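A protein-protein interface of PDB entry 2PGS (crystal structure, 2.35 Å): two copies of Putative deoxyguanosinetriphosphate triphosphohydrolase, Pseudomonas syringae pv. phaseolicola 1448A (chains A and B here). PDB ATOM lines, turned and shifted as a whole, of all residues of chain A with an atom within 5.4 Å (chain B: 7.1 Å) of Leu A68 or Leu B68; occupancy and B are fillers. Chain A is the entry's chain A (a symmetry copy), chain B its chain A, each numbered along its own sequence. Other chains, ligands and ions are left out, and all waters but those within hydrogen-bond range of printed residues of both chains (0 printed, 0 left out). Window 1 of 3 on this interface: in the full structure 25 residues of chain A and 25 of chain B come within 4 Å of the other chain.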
ATOM      1  N   ILE A  37       3.453  -1.184  30.356  1.00  0.00           N
ATOM      2  CA  ILE A  37       2.880  -1.955  29.267  1.00  0.00           C
ATOM      3  C   ILE A  37       1.357  -1.918  29.216  1.00  0.00           C
ATOM      4  O   ILE A  37       0.780  -1.875  28.128  1.00  0.00           O
ATOM      5  CB  ILE A  37       3.421  -3.417  29.285  1.00  0.00           C
ATOM      6  CG1 ILE A  37       4.857  -3.399  28.737  1.00  0.00           C
ATOM      7  CG2 ILE A  37       2.537  -4.343  28.463  1.00  0.00           C
ATOM      8  CD1 ILE A  37       5.398  -4.726  28.382  1.00  0.00           C
ATOM      9  N   PHE A  42       1.052   3.959  26.500  1.00  0.00           N
ATOM     10  CA  PHE A  42       1.983   3.042  25.848  1.00  0.00           C
ATOM     11  C   PHE A  42       1.290   2.325  24.694  1.00  0.00           C
ATOM     12  O   PHE A  42       1.821   2.270  23.585  1.00  0.00           O
ATOM     13  CB  PHE A  42       2.503   1.996  26.848  1.00  0.00           C
ATOM     14  CG  PHE A  42       3.507   1.050  26.263  1.00  0.00           C
ATOM     15  CD1 PHE A  42       4.815   1.467  26.000  1.00  0.00           C
ATOM     16  CD2 PHE A  42       3.145  -0.257  25.951  1.00  0.00           C
ATOM     17  CE1 PHE A  42       5.737   0.582  25.433  1.00  0.00           C
ATOM     18  CE2 PHE A  42       4.052  -1.150  25.384  1.00  0.00           C
ATOM     19  CZ  PHE A  42       5.352  -0.736  25.121  1.00  0.00           C
ATOM     20  N   ARG A  63       6.150   3.391  16.543  1.00  0.00           N
ATOM     21  CA  ARG A  63       6.906   3.829  17.695  1.00  0.00           C
ATOM     22  C   ARG A  63       6.850   2.735  18.762  1.00  0.00           C
ATOM     23  O   ARG A  63       7.722   2.663  19.619  1.00  0.00           O
ATOM     24  CB  ARG A  63       6.354   5.156  18.222  1.00  0.00           C
ATOM     25  CG  ARG A  63       6.721   6.341  17.313  1.00  0.00           C
ATOM     26  CD  ARG A  63       5.860   7.562  17.569  1.00  0.00           C
ATOM     27  NE  ARG A  63       5.876   7.936  18.975  1.00  0.00           N
ATOM     28  CZ  ARG A  63       5.215   8.971  19.485  1.00  0.00           C
ATOM     29  NH1 ARG A  63       4.478   9.745  18.695  1.00  0.00           N
ATOM     30  NH2 ARG A  63       5.288   9.226  20.791  1.00  0.00           N
ATOM     31  N   LEU A  64       5.844   1.867  18.693  1.00  0.00           N
ATOM     32  CA  LEU A  64       5.742   0.781  19.666  1.00  0.00           C
ATOM     33  C   LEU A  64       6.784  -0.316  19.397  1.00  0.00           C
ATOM     34  O   LEU A  64       7.441  -0.779  20.321  1.00  0.00           O
ATOM     35  CB  LEU A  64       4.339   0.167  19.652  1.00  0.00           C
ATOM     36  CG  LEU A  64       4.104  -1.140  20.425  1.00  0.00           C
ATOM     37  CD1 LEU A  64       4.527  -1.006  21.881  1.00  0.00           C
ATOM     38  CD2 LEU A  64       2.614  -1.498  20.344  1.00  0.00           C
ATOM     39  N   THR A  65       6.937  -0.738  18.144  1.00  0.00           N
ATOM     40  CA  THR A  65       7.914  -1.781  17.855  1.00  0.00           C
ATOM     41  C   THR A  65       9.309  -1.227  18.090  1.00  0.00           C
ATOM     42  O   THR A  65      10.199  -1.947  18.529  1.00  0.00           O
ATOM     43  CB  THR A  65       7.768  -2.311  16.419  1.00  0.00           C
ATOM     44  OG1 THR A  65       7.779  -1.216  15.492  1.00  0.00           O
ATOM     45  CG2 THR A  65       6.458  -3.073  16.294  1.00  0.00           C
ATOM     46  N   HIS A  66       9.502   0.059  17.821  1.00  0.00           N
ATOM     47  CA  HIS A  66      10.805   0.654  18.076  1.00  0.00           C
ATOM     48  C   HIS A  66      11.046   0.573  19.594  1.00  0.00           C
ATOM     49  O   HIS A  66      12.084   0.087  20.041  1.00  0.00           O
ATOM     50  CB  HIS A  66      10.856   2.113  17.618  1.00  0.00           C
ATOM     51  CG  HIS A  66      12.116   2.819  18.021  1.00  0.00           C
ATOM     52  ND1 HIS A  66      13.347   2.522  17.469  1.00  0.00           N
ATOM     53  CD2 HIS A  66      12.345   3.758  18.973  1.00  0.00           C
ATOM     54  CE1 HIS A  66      14.279   3.248  18.063  1.00  0.00           C
ATOM     55  NE2 HIS A  66      13.697   4.006  18.980  1.00  0.00           N
ATOM     56  N   SER A  67      10.084   1.039  20.388  1.00  0.00           N
ATOM     57  CA  SER A  67      10.216   0.969  21.849  1.00  0.00           C
ATOM     58  C   SER A  67      10.538  -0.451  22.350  1.00  0.00           C
ATOM     59  O   SER A  67      11.400  -0.625  23.212  1.00  0.00           O
ATOM     60  CB  SER A  67       8.940   1.461  22.523  1.00  0.00           C
ATOM     61  OG  SER A  67       8.835   2.861  22.401  1.00  0.00           O
ATOM     62  N   LEU A  68       9.853  -1.458  21.820  1.00  0.00           N
ATOM     63  CA  LEU A  68      10.118  -2.839  22.236  1.00  0.00           C
ATOM     64  C   LEU A  68      11.565  -3.249  21.954  1.00  0.00           C
ATOM     65  O   LEU A  68      12.239  -3.799  22.830  1.00  0.00           O
ATOM     66  CB  LEU A  68       9.167  -3.806  21.524  1.00  0.00           C
ATOM     67  CG  LEU A  68       7.687  -3.630  21.873  1.00  0.00           C
ATOM     68  CD1 LEU A  68       6.829  -4.562  21.022  1.00  0.00           C
ATOM     69  CD2 LEU A  68       7.491  -3.930  23.355  1.00  0.00           C
ATOM     70  N   GLU A  69      12.040  -2.983  20.736  1.00  0.00           N
ATOM     71  CA  GLU A  69      13.409  -3.339  20.365  1.00  0.00           C
ATOM     72  C   GLU A  69      14.432  -2.649  21.270  1.00  0.00           C
ATOM     73  O   GLU A  69      15.326  -3.295  21.822  1.00  0.00           O
ATOM     74  CB  GLU A  69      13.645  -3.002  18.893  1.00  0.00           C
ATOM     75  CG  GLU A  69      12.751  -3.838  17.978  1.00  0.00           C
ATOM     76  CD  GLU A  69      12.525  -3.214  16.601  1.00  0.00           C
ATOM     77  OE1 GLU A  69      12.352  -1.969  16.519  1.00  0.00           O
ATOM     78  OE2 GLU A  69      12.500  -3.976  15.602  1.00  0.00           O
ATOM     79  N   VAL A  70      14.284  -1.343  21.441  1.00  0.00           N
ATOM     80  CA  VAL A  70      15.172  -0.596  22.311  1.00  0.00           C
ATOM     81  C   VAL A  70      15.172  -1.191  23.736  1.00  0.00           C
ATOM     82  O   VAL A  70      16.209  -1.235  24.400  1.00  0.00           O
ATOM     83  CB  VAL A  70      14.739   0.887  22.370  1.00  0.00           C
ATOM     84  CG1 VAL A  70      15.595   1.652  23.377  1.00  0.00           C
ATOM     85  CG2 VAL A  70      14.856   1.514  20.979  1.00  0.00           C
ATOM     86  N   SER A  71      14.015  -1.654  24.206  1.00  0.00           N
ATOM     87  CA  SER A  71      13.942  -2.219  25.549  1.00  0.00           C
ATOM     88  C   SER A  71      14.706  -3.543  25.657  1.00  0.00           C
ATOM     89  O   SER A  71      15.185  -3.878  26.728  1.00  0.00           O
ATOM     90  CB  SER A  71      12.480  -2.400  25.991  1.00  0.00           C
ATOM     91  OG  SER A  71      11.891  -3.559  25.428  1.00  0.00           O
ATOM     92  N   CYS A  72      14.817  -4.293  24.561  1.00  0.00           N
ATOM     93  CA  CYS A  72      15.570  -5.547  24.580  1.00  0.00           C
ATOM     94  C   CYS A  72      17.052  -5.218  24.754  1.00  0.00           C
ATOM     95  O   CYS A  72      17.728  -5.771  25.620  1.00  0.00           O
ATOM     96  CB  CYS A  72      15.381  -6.315  23.271  1.00  0.00           C
ATOM     97  SG  CYS A  72      13.751  -7.029  23.123  1.00  0.00           S
ATOM     98  N   LEU A 107      10.964   1.508  27.745  1.00  0.00           N
ATOM     99  CA  LEU A 107       9.573   1.399  27.292  1.00  0.00           C
ATOM    100  C   LEU A 107       8.812   2.723  27.438  1.00  0.00           C
ATOM    101  O   LEU A 107       7.906   3.037  26.648  1.00  0.00           O
ATOM    102  CB  LEU A 107       8.841   0.297  28.062  1.00  0.00           C
ATOM    103  CG  LEU A 107       9.243  -1.153  27.752  1.00  0.00           C
ATOM    104  CD1 LEU A 107       8.817  -2.067  28.907  1.00  0.00           C
ATOM    105  CD2 LEU A 107       8.604  -1.597  26.435  1.00  0.00           C
ATOM    106  N   HIS B  33      13.665 -14.515  23.837  1.00  0.00           N
ATOM    107  CA  HIS B  33      12.814 -13.335  23.915  1.00  0.00           C
ATOM    108  C   HIS B  33      13.115 -12.307  22.806  1.00  0.00           C
ATOM    109  O   HIS B  33      12.222 -11.920  22.044  1.00  0.00           O
ATOM    110  CB  HIS B  33      12.974 -12.717  25.312  1.00  0.00           C
ATOM    111  CG  HIS B  33      12.425 -11.335  25.442  1.00  0.00           C
ATOM    112  ND1 HIS B  33      13.044 -10.235  24.889  1.00  0.00           N
ATOM    113  CD2 HIS B  33      11.332 -10.869  26.088  1.00  0.00           C
ATOM    114  CE1 HIS B  33      12.357  -9.149  25.193  1.00  0.00           C
ATOM    115  NE2 HIS B  33      11.312  -9.506  25.919  1.00  0.00           N
ATOM    116  N   ASP B  34      14.375 -11.889  22.710  1.00  0.00           N
ATOM    117  CA  ASP B  34      14.795 -10.914  21.704  1.00  0.00           C
ATOM    118  C   ASP B  34      14.592 -11.384  20.255  1.00  0.00           C
ATOM    119  O   ASP B  34      14.168 -10.612  19.388  1.00  0.00           O
ATOM    120  CB  ASP B  34      16.267 -10.531  21.916  1.00  0.00           C
ATOM    121  CG  ASP B  34      16.502  -9.761  23.221  1.00  0.00           C
ATOM    122  OD1 ASP B  34      15.542  -9.526  23.991  1.00  0.00           O
ATOM    123  OD2 ASP B  34      17.660  -9.381  23.486  1.00  0.00           O
ATOM    124  N   ILE B  37      11.010 -10.842  19.504  1.00  0.00           N
ATOM    125  CA  ILE B  37      10.644  -9.443  19.380  1.00  0.00           C
ATOM    126  C   ILE B  37      11.132  -8.787  18.093  1.00  0.00           C
ATOM    127  O   ILE B  37      10.418  -7.965  17.513  1.00  0.00           O
ATOM    128  CB  ILE B  37      11.093  -8.643  20.640  1.00  0.00           C
ATOM    129  CG1 ILE B  37      10.116  -8.969  21.782  1.00  0.00           C
ATOM    130  CG2 ILE B  37      11.125  -7.147  20.363  1.00  0.00           C
ATOM    131  CD1 ILE B  37      10.198  -8.058  22.942  1.00  0.00           C
ATOM    132  N   PHE B  38      12.322  -9.162  17.630  1.00  0.00           N
ATOM    133  CA  PHE B  38      12.858  -8.590  16.397  1.00  0.00           C
ATOM    134  C   PHE B  38      12.317  -9.242  15.109  1.00  0.00           C
ATOM    135  O   PHE B  38      12.486  -8.687  14.027  1.00  0.00           O
ATOM    136  CB  PHE B  38      14.400  -8.654  16.393  1.00  0.00           C
ATOM    137  CG  PHE B  38      15.058  -7.562  17.214  1.00  0.00           C
ATOM    138  CD1 PHE B  38      15.083  -7.626  18.601  1.00  0.00           C
ATOM    139  CD2 PHE B  38      15.618  -6.451  16.597  1.00  0.00           C
ATOM    140  CE1 PHE B  38      15.653  -6.596  19.359  1.00  0.00           C
ATOM    141  CE2 PHE B  38      16.187  -5.419  17.349  1.00  0.00           C
ATOM    142  CZ  PHE B  38      16.204  -5.496  18.735  1.00  0.00           C
ATOM    143  N   PHE B  42       6.466 -11.338  14.386  1.00  0.00           N
ATOM    144  CA  PHE B  42       5.985 -10.722  15.621  1.00  0.00           C
ATOM    145  C   PHE B  42       5.586  -9.273  15.363  1.00  0.00           C
ATOM    146  O   PHE B  42       4.498  -8.847  15.754  1.00  0.00           O
ATOM    147  CB  PHE B  42       7.077 -10.754  16.703  1.00  0.00           C
ATOM    148  CG  PHE B  42       6.639 -10.187  18.020  1.00  0.00           C
ATOM    149  CD1 PHE B  42       5.773 -10.900  18.853  1.00  0.00           C
ATOM    150  CD2 PHE B  42       7.071  -8.927  18.421  1.00  0.00           C
ATOM    151  CE1 PHE B  42       5.353 -10.351  20.069  1.00  0.00           C
ATOM    152  CE2 PHE B  42       6.659  -8.366  19.629  1.00  0.00           C
ATOM    153  CZ  PHE B  42       5.798  -9.073  20.458  1.00  0.00           C
ATOM    154  N   THR B  62      -4.573  -4.409  19.607  1.00  0.00           N
ATOM    155  CA  THR B  62      -4.182  -5.339  18.551  1.00  0.00           C
ATOM    156  C   THR B  62      -3.696  -6.675  19.110  1.00  0.00           C
ATOM    157  O   THR B  62      -3.603  -6.872  20.323  1.00  0.00           O
ATOM    158  CB  THR B  62      -3.023  -4.766  17.712  1.00  0.00           C
ATOM    159  OG1 THR B  62      -1.854  -4.671  18.541  1.00  0.00           O
ATOM    160  CG2 THR B  62      -3.372  -3.369  17.160  1.00  0.00           C
ATOM    161  N   ARG B  63      -3.371  -7.597  18.220  1.00  0.00           N
ATOM    162  CA  ARG B  63      -2.875  -8.873  18.687  1.00  0.00           C
ATOM    163  C   ARG B  63      -1.501  -8.662  19.323  1.00  0.00           C
ATOM    164  O   ARG B  63      -1.072  -9.460  20.146  1.00  0.00           O
ATOM    165  CB  ARG B  63      -2.811  -9.875  17.530  1.00  0.00           C
ATOM    166  CG  ARG B  63      -4.204 -10.373  17.113  1.00  0.00           C
ATOM    167  CD  ARG B  63      -4.208 -11.016  15.739  1.00  0.00           C
ATOM    168  NE  ARG B  63      -3.208 -12.068  15.645  1.00  0.00           N
ATOM    169  CZ  ARG B  63      -2.993 -12.805  14.560  1.00  0.00           C
ATOM    170  NH1 ARG B  63      -3.717 -12.602  13.462  1.00  0.00           N
ATOM    171  NH2 ARG B  63      -2.046 -13.743  14.571  1.00  0.00           N
ATOM    172  N   LEU B  64      -0.825  -7.573  18.966  1.00  0.00           N
ATOM    173  CA  LEU B  64       0.484  -7.295  19.552  1.00  0.00           C
ATOM    174  C   LEU B  64       0.359  -6.811  21.005  1.00  0.00           C
ATOM    175  O   LEU B  64       1.089  -7.276  21.872  1.00  0.00           O
ATOM    176  CB  LEU B  64       1.239  -6.247  18.730  1.00  0.00           C
ATOM    177  CG  LEU B  64       2.526  -5.644  19.315  1.00  0.00           C
ATOM    178  CD1 LEU B  64       3.524  -6.729  19.694  1.00  0.00           C
ATOM    179  CD2 LEU B  64       3.146  -4.704  18.272  1.00  0.00           C
ATOM    180  N   THR B  65      -0.553  -5.882  21.277  1.00  0.00           N
ATOM    181  CA  THR B  65      -0.695  -5.397  22.645  1.00  0.00           C
ATOM    182  C   THR B  65      -1.238  -6.521  23.511  1.00  0.00           C
ATOM    183  O   THR B  65      -0.885  -6.634  24.680  1.00  0.00           O
ATOM    184  CB  THR B  65      -1.606  -4.160  22.716  1.00  0.00           C
ATOM    185  OG1 THR B  65      -2.847  -4.431  22.052  1.00  0.00           O
ATOM    186  CG2 THR B  65      -0.913  -2.985  22.044  1.00  0.00           C
ATOM    187  N   HIS B  66      -2.082  -7.372  22.938  1.00  0.00           N
ATOM    188  CA  HIS B  66      -2.595  -8.496  23.707  1.00  0.00           C
ATOM    189  C   HIS B  66      -1.386  -9.384  24.060  1.00  0.00           C
ATOM    190  O   HIS B  66      -1.180  -9.732  25.221  1.00  0.00           O
ATOM    191  CB  HIS B  66      -3.617  -9.304  22.907  1.00  0.00           C
ATOM    192  CG  HIS B  66      -4.038 -10.572  23.589  1.00  0.00           C
ATOM    193  ND1 HIS B  66      -4.810 -10.582  24.735  1.00  0.00           N
ATOM    194  CD2 HIS B  66      -3.735 -11.868  23.326  1.00  0.00           C
ATOM    195  CE1 HIS B  66      -4.963 -11.830  25.147  1.00  0.00           C
ATOM    196  NE2 HIS B  66      -4.320 -12.629  24.309  1.00  0.00           N
ATOM    197  N   SER B  67      -0.584  -9.744  23.060  1.00  0.00           N
ATOM    198  CA  SER B  67       0.610 -10.561  23.311  1.00  0.00           C
ATOM    199  C   SER B  67       1.520  -9.966  24.402  1.00  0.00           C
ATOM    200  O   SER B  67       2.000 -10.690  25.275  1.00  0.00           O
ATOM    201  CB  SER B  67       1.414 -10.738  22.030  1.00  0.00           C
ATOM    202  OG  SER B  67       0.751 -11.623  21.156  1.00  0.00           O
ATOM    203  N   LEU B  68       1.759  -8.660  24.356  1.00  0.00           N
ATOM    204  CA  LEU B  68       2.601  -8.020  25.370  1.00  0.00           C
ATOM    205  C   LEU B  68       2.025  -8.193  26.777  1.00  0.00           C
ATOM    206  O   LEU B  68       2.745  -8.576  27.703  1.00  0.00           O
ATOM    207  CB  LEU B  68       2.767  -6.528  25.068  1.00  0.00           C
ATOM    208  CG  LEU B  68       3.511  -6.210  23.768  1.00  0.00           C
ATOM    209  CD1 LEU B  68       3.513  -4.707  23.514  1.00  0.00           C
ATOM    210  CD2 LEU B  68       4.939  -6.735  23.878  1.00  0.00           C
ATOM    211  N   GLU B  69       0.730  -7.910  26.936  1.00  0.00           N
ATOM    212  CA  GLU B  69       0.084  -8.039  28.243  1.00  0.00           C
ATOM    213  C   GLU B  69       0.173  -9.472  28.773  1.00  0.00           C
ATOM    214  O   GLU B  69       0.587  -9.702  29.912  1.00  0.00           O
ATOM    215  CB  GLU B  69      -1.365  -7.564  28.148  1.00  0.00           C
ATOM    216  CG  GLU B  69      -1.444  -6.077  27.805  1.00  0.00           C
ATOM    217  CD  GLU B  69      -2.773  -5.660  27.173  1.00  0.00           C
ATOM    218  OE1 GLU B  69      -3.312  -6.427  26.334  1.00  0.00           O
ATOM    219  OE2 GLU B  69      -3.264  -4.552  27.505  1.00  0.00           O
ATOM    220  N   VAL B  70      -0.194 -10.434  27.938  1.00  0.00           N
ATOM    221  CA  VAL B  70      -0.111 -11.830  28.322  1.00  0.00           C
ATOM    222  C   VAL B  70       1.326 -12.196  28.752  1.00  0.00           C
ATOM    223  O   VAL B  70       1.524 -12.979  29.683  1.00  0.00           O
ATOM    224  CB  VAL B  70      -0.543 -12.734  27.144  1.00  0.00           C
ATOM    225  CG1 VAL B  70      -0.345 -14.205  27.500  1.00  0.00           C
ATOM    226  CG2 VAL B  70      -2.008 -12.460  26.794  1.00  0.00           C
ATOM    227  N   SER B  71       2.329 -11.630  28.084  1.00  0.00           N
ATOM    228  CA  SER B  71       3.711 -11.942  28.432  1.00  0.00           C
ATOM    229  C   SER B  71       4.096 -11.386  29.808  1.00  0.00           C
ATOM    230  O   SER B  71       4.955 -11.947  30.466  1.00  0.00           O
ATOM    231  CB  SER B  71       4.679 -11.430  27.353  1.00  0.00           C
ATOM    232  OG  SER B  71       4.921 -10.039  27.467  1.00  0.00           O
ATOM    233  N   CYS B  72       3.468 -10.291  30.238  1.00  0.00           N
ATOM    234  CA  CYS B  72       3.753  -9.732  31.559  1.00  0.00           C
ATOM    235  C   CYS B  72       3.225 -10.699  32.617  1.00  0.00           C
ATOM    236  O   CYS B  72       3.938 -11.076  33.546  1.00  0.00           O
ATOM    237  CB  CYS B  72       3.065  -8.377  31.736  1.00  0.00           C
ATOM    238  SG  CYS B  72       3.834  -7.086  30.769  1.00  0.00           S
ATOM    239  N   VAL B  73       1.961 -11.077  32.457  1.00  0.00           N
ATOM    240  CA  VAL B  73       1.290 -12.006  33.348  1.00  0.00           C
ATOM    241  C   VAL B  73       1.979 -13.366  33.280  1.00  0.00           C
ATOM    242  O   VAL B  73       2.084 -14.072  34.282  1.00  0.00           O
ATOM    243  CB  VAL B  73      -0.184 -12.156  32.939  1.00  0.00           C
ATOM    244  CG1 VAL B  73      -0.842 -13.289  33.706  1.00  0.00           C
ATOM    245  CG2 VAL B  73      -0.899 -10.847  33.184  1.00  0.00           C
ATOM    246  N   GLY B  74       2.448 -13.729  32.089  1.00  0.00           N
ATOM    247  CA  GLY B  74       3.145 -14.993  31.931  1.00  0.00           C
ATOM    248  C   GLY B  74       4.434 -14.990  32.738  1.00  0.00           C
ATOM    249  O   GLY B  74       4.681 -15.915  33.507  1.00  0.00           O
ATOM    250  N   GLN B 103       7.542 -16.059  29.462  1.00  0.00           N
ATOM    251  CA  GLN B 103       7.299 -14.786  28.798  1.00  0.00           C
ATOM    252  C   GLN B 103       7.549 -14.924  27.298  1.00  0.00           C
ATOM    253  O   GLN B 103       6.795 -14.396  26.481  1.00  0.00           O
ATOM    254  CB  GLN B 103       8.220 -13.703  29.355  1.00  0.00           C
ATOM    255  CG  GLN B 103       7.865 -12.315  28.885  1.00  0.00           C
ATOM    256  CD  GLN B 103       8.709 -11.235  29.548  1.00  0.00           C
ATOM    257  OE1 GLN B 103       9.929 -11.292  29.520  1.00  0.00           O
ATOM    258  NE2 GLN B 103       8.055 -10.240  30.138  1.00  0.00           N
ATOM    259  N   CYS B 106       4.870 -16.898  25.582  1.00  0.00           N
ATOM    260  CA  CYS B 106       3.702 -16.018  25.513  1.00  0.00           C
ATOM    261  C   CYS B 106       3.800 -15.047  24.320  1.00  0.00           C
ATOM    262  O   CYS B 106       2.798 -14.753  23.655  1.00  0.00           O
ATOM    263  CB  CYS B 106       3.562 -15.205  26.808  1.00  0.00           C
ATOM    264  SG  CYS B 106       2.887 -16.138  28.253  1.00  0.00           S
ATOM    265  N   LEU B 107       4.998 -14.537  24.051  1.00  0.00           N
ATOM    266  CA  LEU B 107       5.168 -13.611  22.927  1.00  0.00           C
ATOM    267  C   LEU B 107       4.993 -14.309  21.572  1.00  0.00           C
ATOM    268  O   LEU B 107       4.529 -13.706  20.591  1.00  0.00           O
ATOM    269  CB  LEU B 107       6.542 -12.938  22.986  1.00  0.00           C
ATOM    270  CG  LEU B 107       6.763 -11.905  24.102  1.00  0.00           C
ATOM    271  CD1 LEU B 107       8.265 -11.712  24.338  1.00  0.00           C
ATOM    272  CD2 LEU B 107       6.091 -10.584  23.724  1.00  0.00           C
ATOM    273  N   CYS B 246      -5.796 -12.597  30.597  1.00  0.00           N
ATOM    274  CA  CYS B 246      -5.789 -11.321  29.884  1.00  0.00           C
ATOM    275  C   CYS B 246      -6.974 -11.106  28.953  1.00  0.00           C
ATOM    276  O   CYS B 246      -7.462  -9.987  28.825  1.00  0.00           O
ATOM    277  CB  CYS B 246      -4.485 -11.148  29.110  1.00  0.00           C
ATOM    278  SG  CYS B 246      -3.044 -10.842  30.175  1.00  0.00           S
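Hydrophobic or aromatic side chains of chain A within 4 Å of the printed part of chain B: Ile A37, Leu A64 and Leu A68.
Of the 22 printed residues of chain B, 7 touch a printed residue of chain A.
Among the printed residues, no Asp or Glu carboxylate lies within 4 Å of a Lys or Arg side-chain nitrogen of the other chain.
Ile A37 touches Cys B72, and with the chains exchanged Cys A72 touches Ile B37.
Leu B64 touches its own counterpart, Leu A64.
Leu A68 touches its own counterpart, Leu B68.
Positions printed for both chains: 37, 42, 63, 64, 65, 66, 67, 68, 69, 70, 71, 72 and 107.
Of the 8 pairs that touch across the chains among the printed residues, 4 have their exchanged pair printed and touching as well.
O of Leu B68 lies within hydrogen-bond range of OG of Ser B71, 2.6 Å away.
The backbone carbonyl oxygen of Leu B68 is in hydrogen-bond range of the side-chain sulfur of Cys B72, 3.6 Å away.
OG1 of Thr B62 lies close to N of Leu B64 (3.1 Å).
The side-chain sulfur (SG) of Cys A72 sits at hydrogen-bond distance from the backbone carbonyl oxygen (O) of Leu A68, 3.6 Å away.
ND1 of His B33 is in hydrogen-bond range of OD1 of Asp B34, at 2.7 Å.
O of Leu A68 lies within hydrogen-bond range of OG of Ser A71 (2.6 Å).
Among the printed residues, merely in contact across the chains: Glu A69 with Phe B38, Ile A37 with Cys B72, Cys A72 with Ile B37, Leu A68 with Leu B68, Leu A64 with Leu B64 and Cys A72 with Phe B38.
Leu A68 touches just one residue of chain B: Leu B68.
Of the printed residues of chain B, Cys A72 touches His B33 (3.3 Å), Asp B34 (3.2 Å), Ile B37 (3.7 Å) and Phe B38 (3.9 Å).
Printed residues of chain A within 4 Å of Asp B34: Cys A72.
Of the printed residues of chain A, Leu B64 touches Leu A64 (3.9 Å).
Of the printed residues of chain A, Cys B72 touches Ile A37 (3.7 Å).
The side-chain sulfur of Cys A72 is in hydrogen-bond range of the side-chain carboxylate of Asp B34, 3.2 Å away.
ND1 of His B33 sits close to SG of Cys A72, 3.7 Å away.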
